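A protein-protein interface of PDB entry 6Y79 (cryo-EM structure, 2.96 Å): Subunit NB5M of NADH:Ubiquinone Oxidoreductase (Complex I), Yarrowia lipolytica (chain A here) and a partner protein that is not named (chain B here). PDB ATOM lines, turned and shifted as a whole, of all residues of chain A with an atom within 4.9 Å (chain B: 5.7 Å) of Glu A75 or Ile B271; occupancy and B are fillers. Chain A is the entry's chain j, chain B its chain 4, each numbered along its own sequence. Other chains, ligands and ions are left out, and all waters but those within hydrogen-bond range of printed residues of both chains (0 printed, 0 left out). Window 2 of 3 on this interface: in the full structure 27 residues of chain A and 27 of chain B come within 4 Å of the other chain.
The side-chain amide oxygen of Asn B406 lies close to the backbone carbonyl oxygen of Ser A74, 3.0 Å away.
The guanidinium group (NH1) of Arg B405 lies within salt-bridge range of the side-chain carboxylate (OE1) of Glu A75.
OG1 of Thr B274 sits at hydrogen-bond distance from O of Ile B271 (3.4 Å).
NH1 of Arg B405 sits at hydrogen-bond distance from OG1 of Thr B274.
Ala A71 touches Asn B406 (O to ND2, 3.97 Å).
CE1 of Tyr A72 touches CG of Pro B275, 3.6 Å away.
O of Ile B271 touches OE1 of Glu A75 (3.6 Å).
OE1 of Glu A75 touches OG1 of Thr B274, 3.7 Å away.
Glu A75 touches Pro B275.
Of the printed residues of chain B, Ala A71 touches Asn B406.
Of the printed residues of chain B, Tyr A72 touches Pro B275.
Glu A75 touches just these residues of chain B: Ile B271 (3.6 Å), Thr B274 (3.7 Å), Pro B275 (3.3 Å) and Arg B405 (2.5 Å).
Gly A76 touches none of the printed residues of chain B.
Ile B271 touches just one residue of chain A: Glu A75.
Printed residues of chain A within 4 Å of Arg B405: Glu A75 (2.5 Å).
Printed residues of chain A within 4 Å of Asn B406: Ala A71 and Ser A74.
Tyr B484 touches none of the printed residues of chain A.
The nearest residue of chain B that does not touch Glu A75 is Asn B406 (5.0 Å).
Of the 14 printed residues of chain B, 5 touch a printed residue of chain A.
Hydrophobic or aromatic side chains of chain B within 4 Å of the printed part of chain A: Pro B275.
Hydrophobic or aromatic side chains of chain A that line the printed part of chain B: Tyr A72.
Along chain A the printed residues that touch a printed residue of chain B span positions 71 to 75.
Among the printed residues, 7 pairs touch across the chains.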
ATOM      1  N   ALA A  71       2.367 -21.835  30.570  1.00  0.00           N
ATOM      2  CA  ALA A  71       3.674 -21.438  30.055  1.00  0.00           C
ATOM      3  C   ALA A  71       3.631 -21.102  28.569  1.00  0.00           C
ATOM      4  O   ALA A  71       4.380 -20.234  28.109  1.00  0.00           O
ATOM      5  CB  ALA A  71       4.698 -22.540  30.318  1.00  0.00           C
ATOM      6  N   TYR A  72       2.779 -21.777  27.795  1.00  0.00           N
ATOM      7  CA  TYR A  72       2.712 -21.451  26.374  1.00  0.00           C
ATOM      8  C   TYR A  72       1.802 -20.260  26.098  1.00  0.00           C
ATOM      9  O   TYR A  72       2.010 -19.560  25.103  1.00  0.00           O
ATOM     10  CB  TYR A  72       2.258 -22.658  25.548  1.00  0.00           C
ATOM     11  CG  TYR A  72       3.290 -23.760  25.423  1.00  0.00           C
ATOM     12  CD1 TYR A  72       4.444 -23.593  24.670  1.00  0.00           C
ATOM     13  CD2 TYR A  72       3.095 -24.979  26.042  1.00  0.00           C
ATOM     14  CE1 TYR A  72       5.373 -24.614  24.565  1.00  0.00           C
ATOM     15  CE2 TYR A  72       4.013 -25.988  25.956  1.00  0.00           C
ATOM     16  CZ  TYR A  72       5.146 -25.804  25.215  1.00  0.00           C
ATOM     17  OH  TYR A  72       6.047 -26.832  25.132  1.00  0.00           O
ATOM     18  N   GLN A  73       0.797 -20.007  26.948  1.00  0.00           N
ATOM     19  CA  GLN A  73      -0.047 -18.836  26.723  1.00  0.00           C
ATOM     20  C   GLN A  73       0.684 -17.536  27.027  1.00  0.00           C
ATOM     21  O   GLN A  73       0.355 -16.496  26.450  1.00  0.00           O
ATOM     22  CB  GLN A  73      -1.317 -18.901  27.571  1.00  0.00           C
ATOM     23  CG  GLN A  73      -2.391 -19.855  27.087  1.00  0.00           C
ATOM     24  CD  GLN A  73      -2.859 -19.572  25.683  1.00  0.00           C
ATOM     25  OE1 GLN A  73      -3.053 -18.419  25.298  1.00  0.00           O
ATOM     26  NE2 GLN A  73      -3.053 -20.630  24.905  1.00  0.00           N
ATOM     27  N   SER A  74       1.668 -17.568  27.920  1.00  0.00           N
ATOM     28  CA  SER A  74       2.246 -16.358  28.496  1.00  0.00           C
ATOM     29  C   SER A  74       3.709 -16.164  28.135  1.00  0.00           C
ATOM     30  O   SER A  74       4.496 -15.756  28.991  1.00  0.00           O
ATOM     31  CB  SER A  74       2.090 -16.385  30.009  1.00  0.00           C
ATOM     32  OG  SER A  74       2.894 -17.407  30.569  1.00  0.00           O
ATOM     33  N   GLU A  75       4.125 -16.428  26.896  1.00  0.00           N
ATOM     34  CA  GLU A  75       5.555 -16.340  26.598  1.00  0.00           C
ATOM     35  C   GLU A  75       5.988 -14.910  26.292  1.00  0.00           C
ATOM     36  O   GLU A  75       6.868 -14.360  26.960  1.00  0.00           O
ATOM     37  CB  GLU A  75       5.941 -17.276  25.452  1.00  0.00           C
ATOM     38  CG  GLU A  75       7.335 -17.802  25.683  1.00  0.00           C
ATOM     39  CD  GLU A  75       8.007 -18.339  24.450  1.00  0.00           C
ATOM     40  OE1 GLU A  75       9.168 -18.789  24.562  1.00  0.00           O
ATOM     41  OE2 GLU A  75       7.374 -18.333  23.380  1.00  0.00           O
ATOM     42  N   GLY A  76       5.389 -14.296  25.284  1.00  0.00           N
ATOM     43  CA  GLY A  76       5.761 -12.941  24.953  1.00  0.00           C
ATOM     44  C   GLY A  76       4.778 -11.918  25.477  1.00  0.00           C
ATOM     45  O   GLY A  76       4.695 -10.811  24.935  1.00  0.00           O
ATOM     46  N   LEU A  77       4.007 -12.282  26.507  1.00  0.00           N
ATOM     47  CA  LEU A  77       3.057 -11.356  27.107  1.00  0.00           C
ATOM     48  C   LEU A  77       3.772 -10.178  27.743  1.00  0.00           C
ATOM     49  O   LEU A  77       3.757  -9.073  27.201  1.00  0.00           O
ATOM     50  CB  LEU A  77       2.203 -12.051  28.169  1.00  0.00           C
ATOM     51  CG  LEU A  77       0.835 -12.656  27.860  1.00  0.00           C
ATOM     52  CD1 LEU A  77       0.247 -13.254  29.116  1.00  0.00           C
ATOM     53  CD2 LEU A  77      -0.103 -11.616  27.306  1.00  0.00           C
ATOM     54  N   ARG A  92       0.256  -8.519  23.590  1.00  0.00           N
ATOM     55  CA  ARG A  92      -0.931  -8.946  22.863  1.00  0.00           C
ATOM     56  C   ARG A  92      -2.179  -8.831  23.732  1.00  0.00           C
ATOM     57  O   ARG A  92      -3.000  -7.936  23.542  1.00  0.00           O
ATOM     58  CB  ARG A  92      -0.769 -10.384  22.369  1.00  0.00           C
ATOM     59  CG  ARG A  92      -0.909 -11.437  23.456  1.00  0.00           C
ATOM     60  CD  ARG A  92      -0.540 -12.811  22.936  1.00  0.00           C
ATOM     61  NE  ARG A  92       0.874 -12.894  22.587  1.00  0.00           N
ATOM     62  CZ  ARG A  92       1.797 -13.482  23.338  1.00  0.00           C
ATOM     63  NH1 ARG A  92       1.462 -14.051  24.487  1.00  0.00           N
ATOM     64  NH2 ARG A  92       3.059 -13.507  22.935  1.00  0.00           N
ATOM     65  N   LEU B 266      22.158 -24.091  18.502  1.00  0.00           N
ATOM     66  CA  LEU B 266      20.734 -24.375  18.524  1.00  0.00           C
ATOM     67  C   LEU B 266      19.941 -23.189  19.038  1.00  0.00           C
ATOM     68  O   LEU B 266      18.958 -23.373  19.742  1.00  0.00           O
ATOM     69  CB  LEU B 266      20.404 -25.585  19.393  1.00  0.00           C
ATOM     70  CG  LEU B 266      20.488 -27.033  18.940  1.00  0.00           C
ATOM     71  CD1 LEU B 266      19.719 -27.152  17.692  1.00  0.00           C
ATOM     72  CD2 LEU B 266      21.871 -27.527  18.759  1.00  0.00           C
ATOM     73  N   CYS B 267      20.355 -21.965  18.687  1.00  0.00           N
ATOM     74  CA  CYS B 267      19.722 -20.752  19.208  1.00  0.00           C
ATOM     75  C   CYS B 267      18.263 -20.647  18.783  1.00  0.00           C
ATOM     76  O   CYS B 267      17.354 -20.505  19.619  1.00  0.00           O
ATOM     77  CB  CYS B 267      20.477 -19.530  18.700  1.00  0.00           C
ATOM     78  SG  CYS B 267      22.191 -19.417  19.180  1.00  0.00           S
ATOM     79  N   GLU B 268      18.029 -20.734  17.478  1.00  0.00           N
ATOM     80  CA  GLU B 268      16.698 -20.636  16.918  1.00  0.00           C
ATOM     81  C   GLU B 268      15.831 -21.828  17.299  1.00  0.00           C
ATOM     82  O   GLU B 268      14.606 -21.728  17.247  1.00  0.00           O
ATOM     83  CB  GLU B 268      16.808 -20.488  15.400  1.00  0.00           C
ATOM     84  CG  GLU B 268      17.424 -19.167  14.941  1.00  0.00           C
ATOM     85  CD  GLU B 268      18.941 -19.183  14.861  1.00  0.00           C
ATOM     86  OE1 GLU B 268      19.544 -20.251  15.061  1.00  0.00           O
ATOM     87  OE2 GLU B 268      19.534 -18.117  14.605  1.00  0.00           O
ATOM     88  N   ALA B 269      16.434 -22.950  17.683  1.00  0.00           N
ATOM     89  CA  ALA B 269      15.659 -24.026  18.283  1.00  0.00           C
ATOM     90  C   ALA B 269      15.317 -23.701  19.727  1.00  0.00           C
ATOM     91  O   ALA B 269      14.160 -23.821  20.136  1.00  0.00           O
ATOM     92  CB  ALA B 269      16.426 -25.341  18.204  1.00  0.00           C
ATOM     93  N   GLN B 270      16.322 -23.262  20.496  1.00  0.00           N
ATOM     94  CA  GLN B 270      16.216 -23.010  21.935  1.00  0.00           C
ATOM     95  C   GLN B 270      15.115 -22.021  22.290  1.00  0.00           C
ATOM     96  O   GLN B 270      14.434 -22.192  23.317  1.00  0.00           O
ATOM     97  CB  GLN B 270      17.554 -22.478  22.436  1.00  0.00           C
ATOM     98  CG  GLN B 270      17.686 -22.295  23.903  1.00  0.00           C
ATOM     99  CD  GLN B 270      17.607 -23.589  24.640  1.00  0.00           C
ATOM    100  OE1 GLN B 270      16.653 -23.836  25.354  1.00  0.00           O
ATOM    101  NE2 GLN B 270      18.603 -24.437  24.461  1.00  0.00           N
ATOM    102  N   ILE B 271      14.931 -20.986  21.464  1.00  0.00           N
ATOM    103  CA  ILE B 271      13.861 -20.024  21.715  1.00  0.00           C
ATOM    104  C   ILE B 271      12.490 -20.686  21.590  1.00  0.00           C
ATOM    105  O   ILE B 271      11.567 -20.379  22.353  1.00  0.00           O
ATOM    106  CB  ILE B 271      14.009 -18.817  20.776  1.00  0.00           C
ATOM    107  CG1 ILE B 271      15.398 -18.212  20.919  1.00  0.00           C
ATOM    108  CG2 ILE B 271      12.991 -17.755  21.091  1.00  0.00           C
ATOM    109  CD1 ILE B 271      15.690 -17.680  22.285  1.00  0.00           C
ATOM    110  N   LEU B 272      12.348 -21.642  20.675  1.00  0.00           N
ATOM    111  CA  LEU B 272      11.082 -22.346  20.526  1.00  0.00           C
ATOM    112  C   LEU B 272      10.785 -23.303  21.671  1.00  0.00           C
ATOM    113  O   LEU B 272       9.634 -23.728  21.814  1.00  0.00           O
ATOM    114  CB  LEU B 272      11.056 -23.138  19.220  1.00  0.00           C
ATOM    115  CG  LEU B 272      10.942 -22.406  17.890  1.00  0.00           C
ATOM    116  CD1 LEU B 272      10.967 -23.398  16.757  1.00  0.00           C
ATOM    117  CD2 LEU B 272       9.694 -21.553  17.833  1.00  0.00           C
ATOM    118  N   TYR B 273      11.776 -23.648  22.484  1.00  0.00           N
ATOM    119  CA  TYR B 273      11.629 -24.737  23.431  1.00  0.00           C
ATOM    120  C   TYR B 273      11.752 -24.351  24.889  1.00  0.00           C
ATOM    121  O   TYR B 273      11.461 -25.193  25.742  1.00  0.00           O
ATOM    122  CB  TYR B 273      12.663 -25.827  23.155  1.00  0.00           C
ATOM    123  CG  TYR B 273      12.307 -26.687  21.993  1.00  0.00           C
ATOM    124  CD1 TYR B 273      11.244 -27.566  22.063  1.00  0.00           C
ATOM    125  CD2 TYR B 273      13.039 -26.633  20.827  1.00  0.00           C
ATOM    126  CE1 TYR B 273      10.916 -28.353  21.001  1.00  0.00           C
ATOM    127  CE2 TYR B 273      12.723 -27.413  19.758  1.00  0.00           C
ATOM    128  CZ  TYR B 273      11.657 -28.275  19.849  1.00  0.00           C
ATOM    129  OH  TYR B 273      11.316 -29.070  18.787  1.00  0.00           O
ATOM    130  N   THR B 274      12.219 -23.143  25.201  1.00  0.00           N
ATOM    131  CA  THR B 274      12.285 -22.718  26.603  1.00  0.00           C
ATOM    132  C   THR B 274      10.991 -22.775  27.432  1.00  0.00           C
ATOM    133  O   THR B 274      11.096 -22.950  28.652  1.00  0.00           O
ATOM    134  CB  THR B 274      12.863 -21.308  26.694  1.00  0.00           C
ATOM    135  OG1 THR B 274      12.304 -20.485  25.667  1.00  0.00           O
ATOM    136  CG2 THR B 274      14.363 -21.344  26.534  1.00  0.00           C
ATOM    137  N   PRO B 275       9.771 -22.661  26.874  1.00  0.00           N
ATOM    138  CA  PRO B 275       8.598 -22.993  27.702  1.00  0.00           C
ATOM    139  C   PRO B 275       8.520 -24.456  28.102  1.00  0.00           C
ATOM    140  O   PRO B 275       8.059 -24.750  29.209  1.00  0.00           O
ATOM    141  CB  PRO B 275       7.409 -22.588  26.818  1.00  0.00           C
ATOM    142  CG  PRO B 275       7.971 -22.367  25.488  1.00  0.00           C
ATOM    143  CD  PRO B 275       9.328 -21.865  25.718  1.00  0.00           C
ATOM    144  N   ASN B 320      17.977 -16.892  28.732  1.00  0.00           N
ATOM    145  CA  ASN B 320      18.389 -15.901  27.730  1.00  0.00           C
ATOM    146  C   ASN B 320      18.853 -14.600  28.380  1.00  0.00           C
ATOM    147  O   ASN B 320      18.756 -13.527  27.795  1.00  0.00           O
ATOM    148  CB  ASN B 320      17.268 -15.648  26.709  1.00  0.00           C
ATOM    149  CG  ASN B 320      17.770 -15.165  25.374  1.00  0.00           C
ATOM    150  OD1 ASN B 320      18.968 -15.112  25.131  1.00  0.00           O
ATOM    151  ND2 ASN B 320      16.846 -14.797  24.499  1.00  0.00           N
ATOM    152  N   ARG B 405      12.561 -14.162  31.752  1.00  0.00           N
ATOM    153  CA  ARG B 405      12.154 -14.909  30.562  1.00  0.00           C
ATOM    154  C   ARG B 405      10.666 -15.259  30.578  1.00  0.00           C
ATOM    155  O   ARG B 405      10.017 -15.230  29.528  1.00  0.00           O
ATOM    156  CB  ARG B 405      13.015 -16.163  30.422  1.00  0.00           C
ATOM    157  CG  ARG B 405      12.783 -16.992  29.163  1.00  0.00           C
ATOM    158  CD  ARG B 405      12.822 -16.169  27.878  1.00  0.00           C
ATOM    159  NE  ARG B 405      12.699 -17.006  26.686  1.00  0.00           N
ATOM    160  CZ  ARG B 405      11.554 -17.511  26.236  1.00  0.00           C
ATOM    161  NH1 ARG B 405      11.537 -18.257  25.140  1.00  0.00           N
ATOM    162  NH2 ARG B 405      10.414 -17.255  26.863  1.00  0.00           N
ATOM    163  N   ASN B 406      10.109 -15.557  31.742  1.00  0.00           N
ATOM    164  CA  ASN B 406       8.678 -15.771  31.906  1.00  0.00           C
ATOM    165  C   ASN B 406       8.298 -15.435  33.341  1.00  0.00           C
ATOM    166  O   ASN B 406       8.707 -16.145  34.266  1.00  0.00           O
ATOM    167  CB  ASN B 406       8.295 -17.211  31.569  1.00  0.00           C
ATOM    168  CG  ASN B 406       6.797 -17.402  31.408  1.00  0.00           C
ATOM    169  OD1 ASN B 406       6.014 -16.461  31.530  1.00  0.00           O
ATOM    170  ND2 ASN B 406       6.393 -18.628  31.126  1.00  0.00           N
ATOM    171  N   TYR B 484      21.040 -14.503  22.940  1.00  0.00           N
ATOM    172  CA  TYR B 484      20.484 -14.382  21.591  1.00  0.00           C
ATOM    173  C   TYR B 484      19.286 -13.430  21.663  1.00  0.00           C
ATOM    174  O   TYR B 484      18.134 -13.860  21.709  1.00  0.00           O
ATOM    175  CB  TYR B 484      20.104 -15.781  21.091  1.00  0.00           C
ATOM    176  CG  TYR B 484      19.639 -15.866  19.667  1.00  0.00           C
ATOM    177  CD1 TYR B 484      20.544 -15.885  18.620  1.00  0.00           C
ATOM    178  CD2 TYR B 484      18.287 -15.950  19.367  1.00  0.00           C
ATOM    179  CE1 TYR B 484      20.119 -15.966  17.323  1.00  0.00           C
ATOM    180  CE2 TYR B 484      17.852 -16.027  18.070  1.00  0.00           C
ATOM    181  CZ  TYR B 484      18.774 -16.035  17.054  1.00  0.00           C
ATOM    182  OH  TYR B 484      18.354 -16.113  15.752  1.00  0.00           O
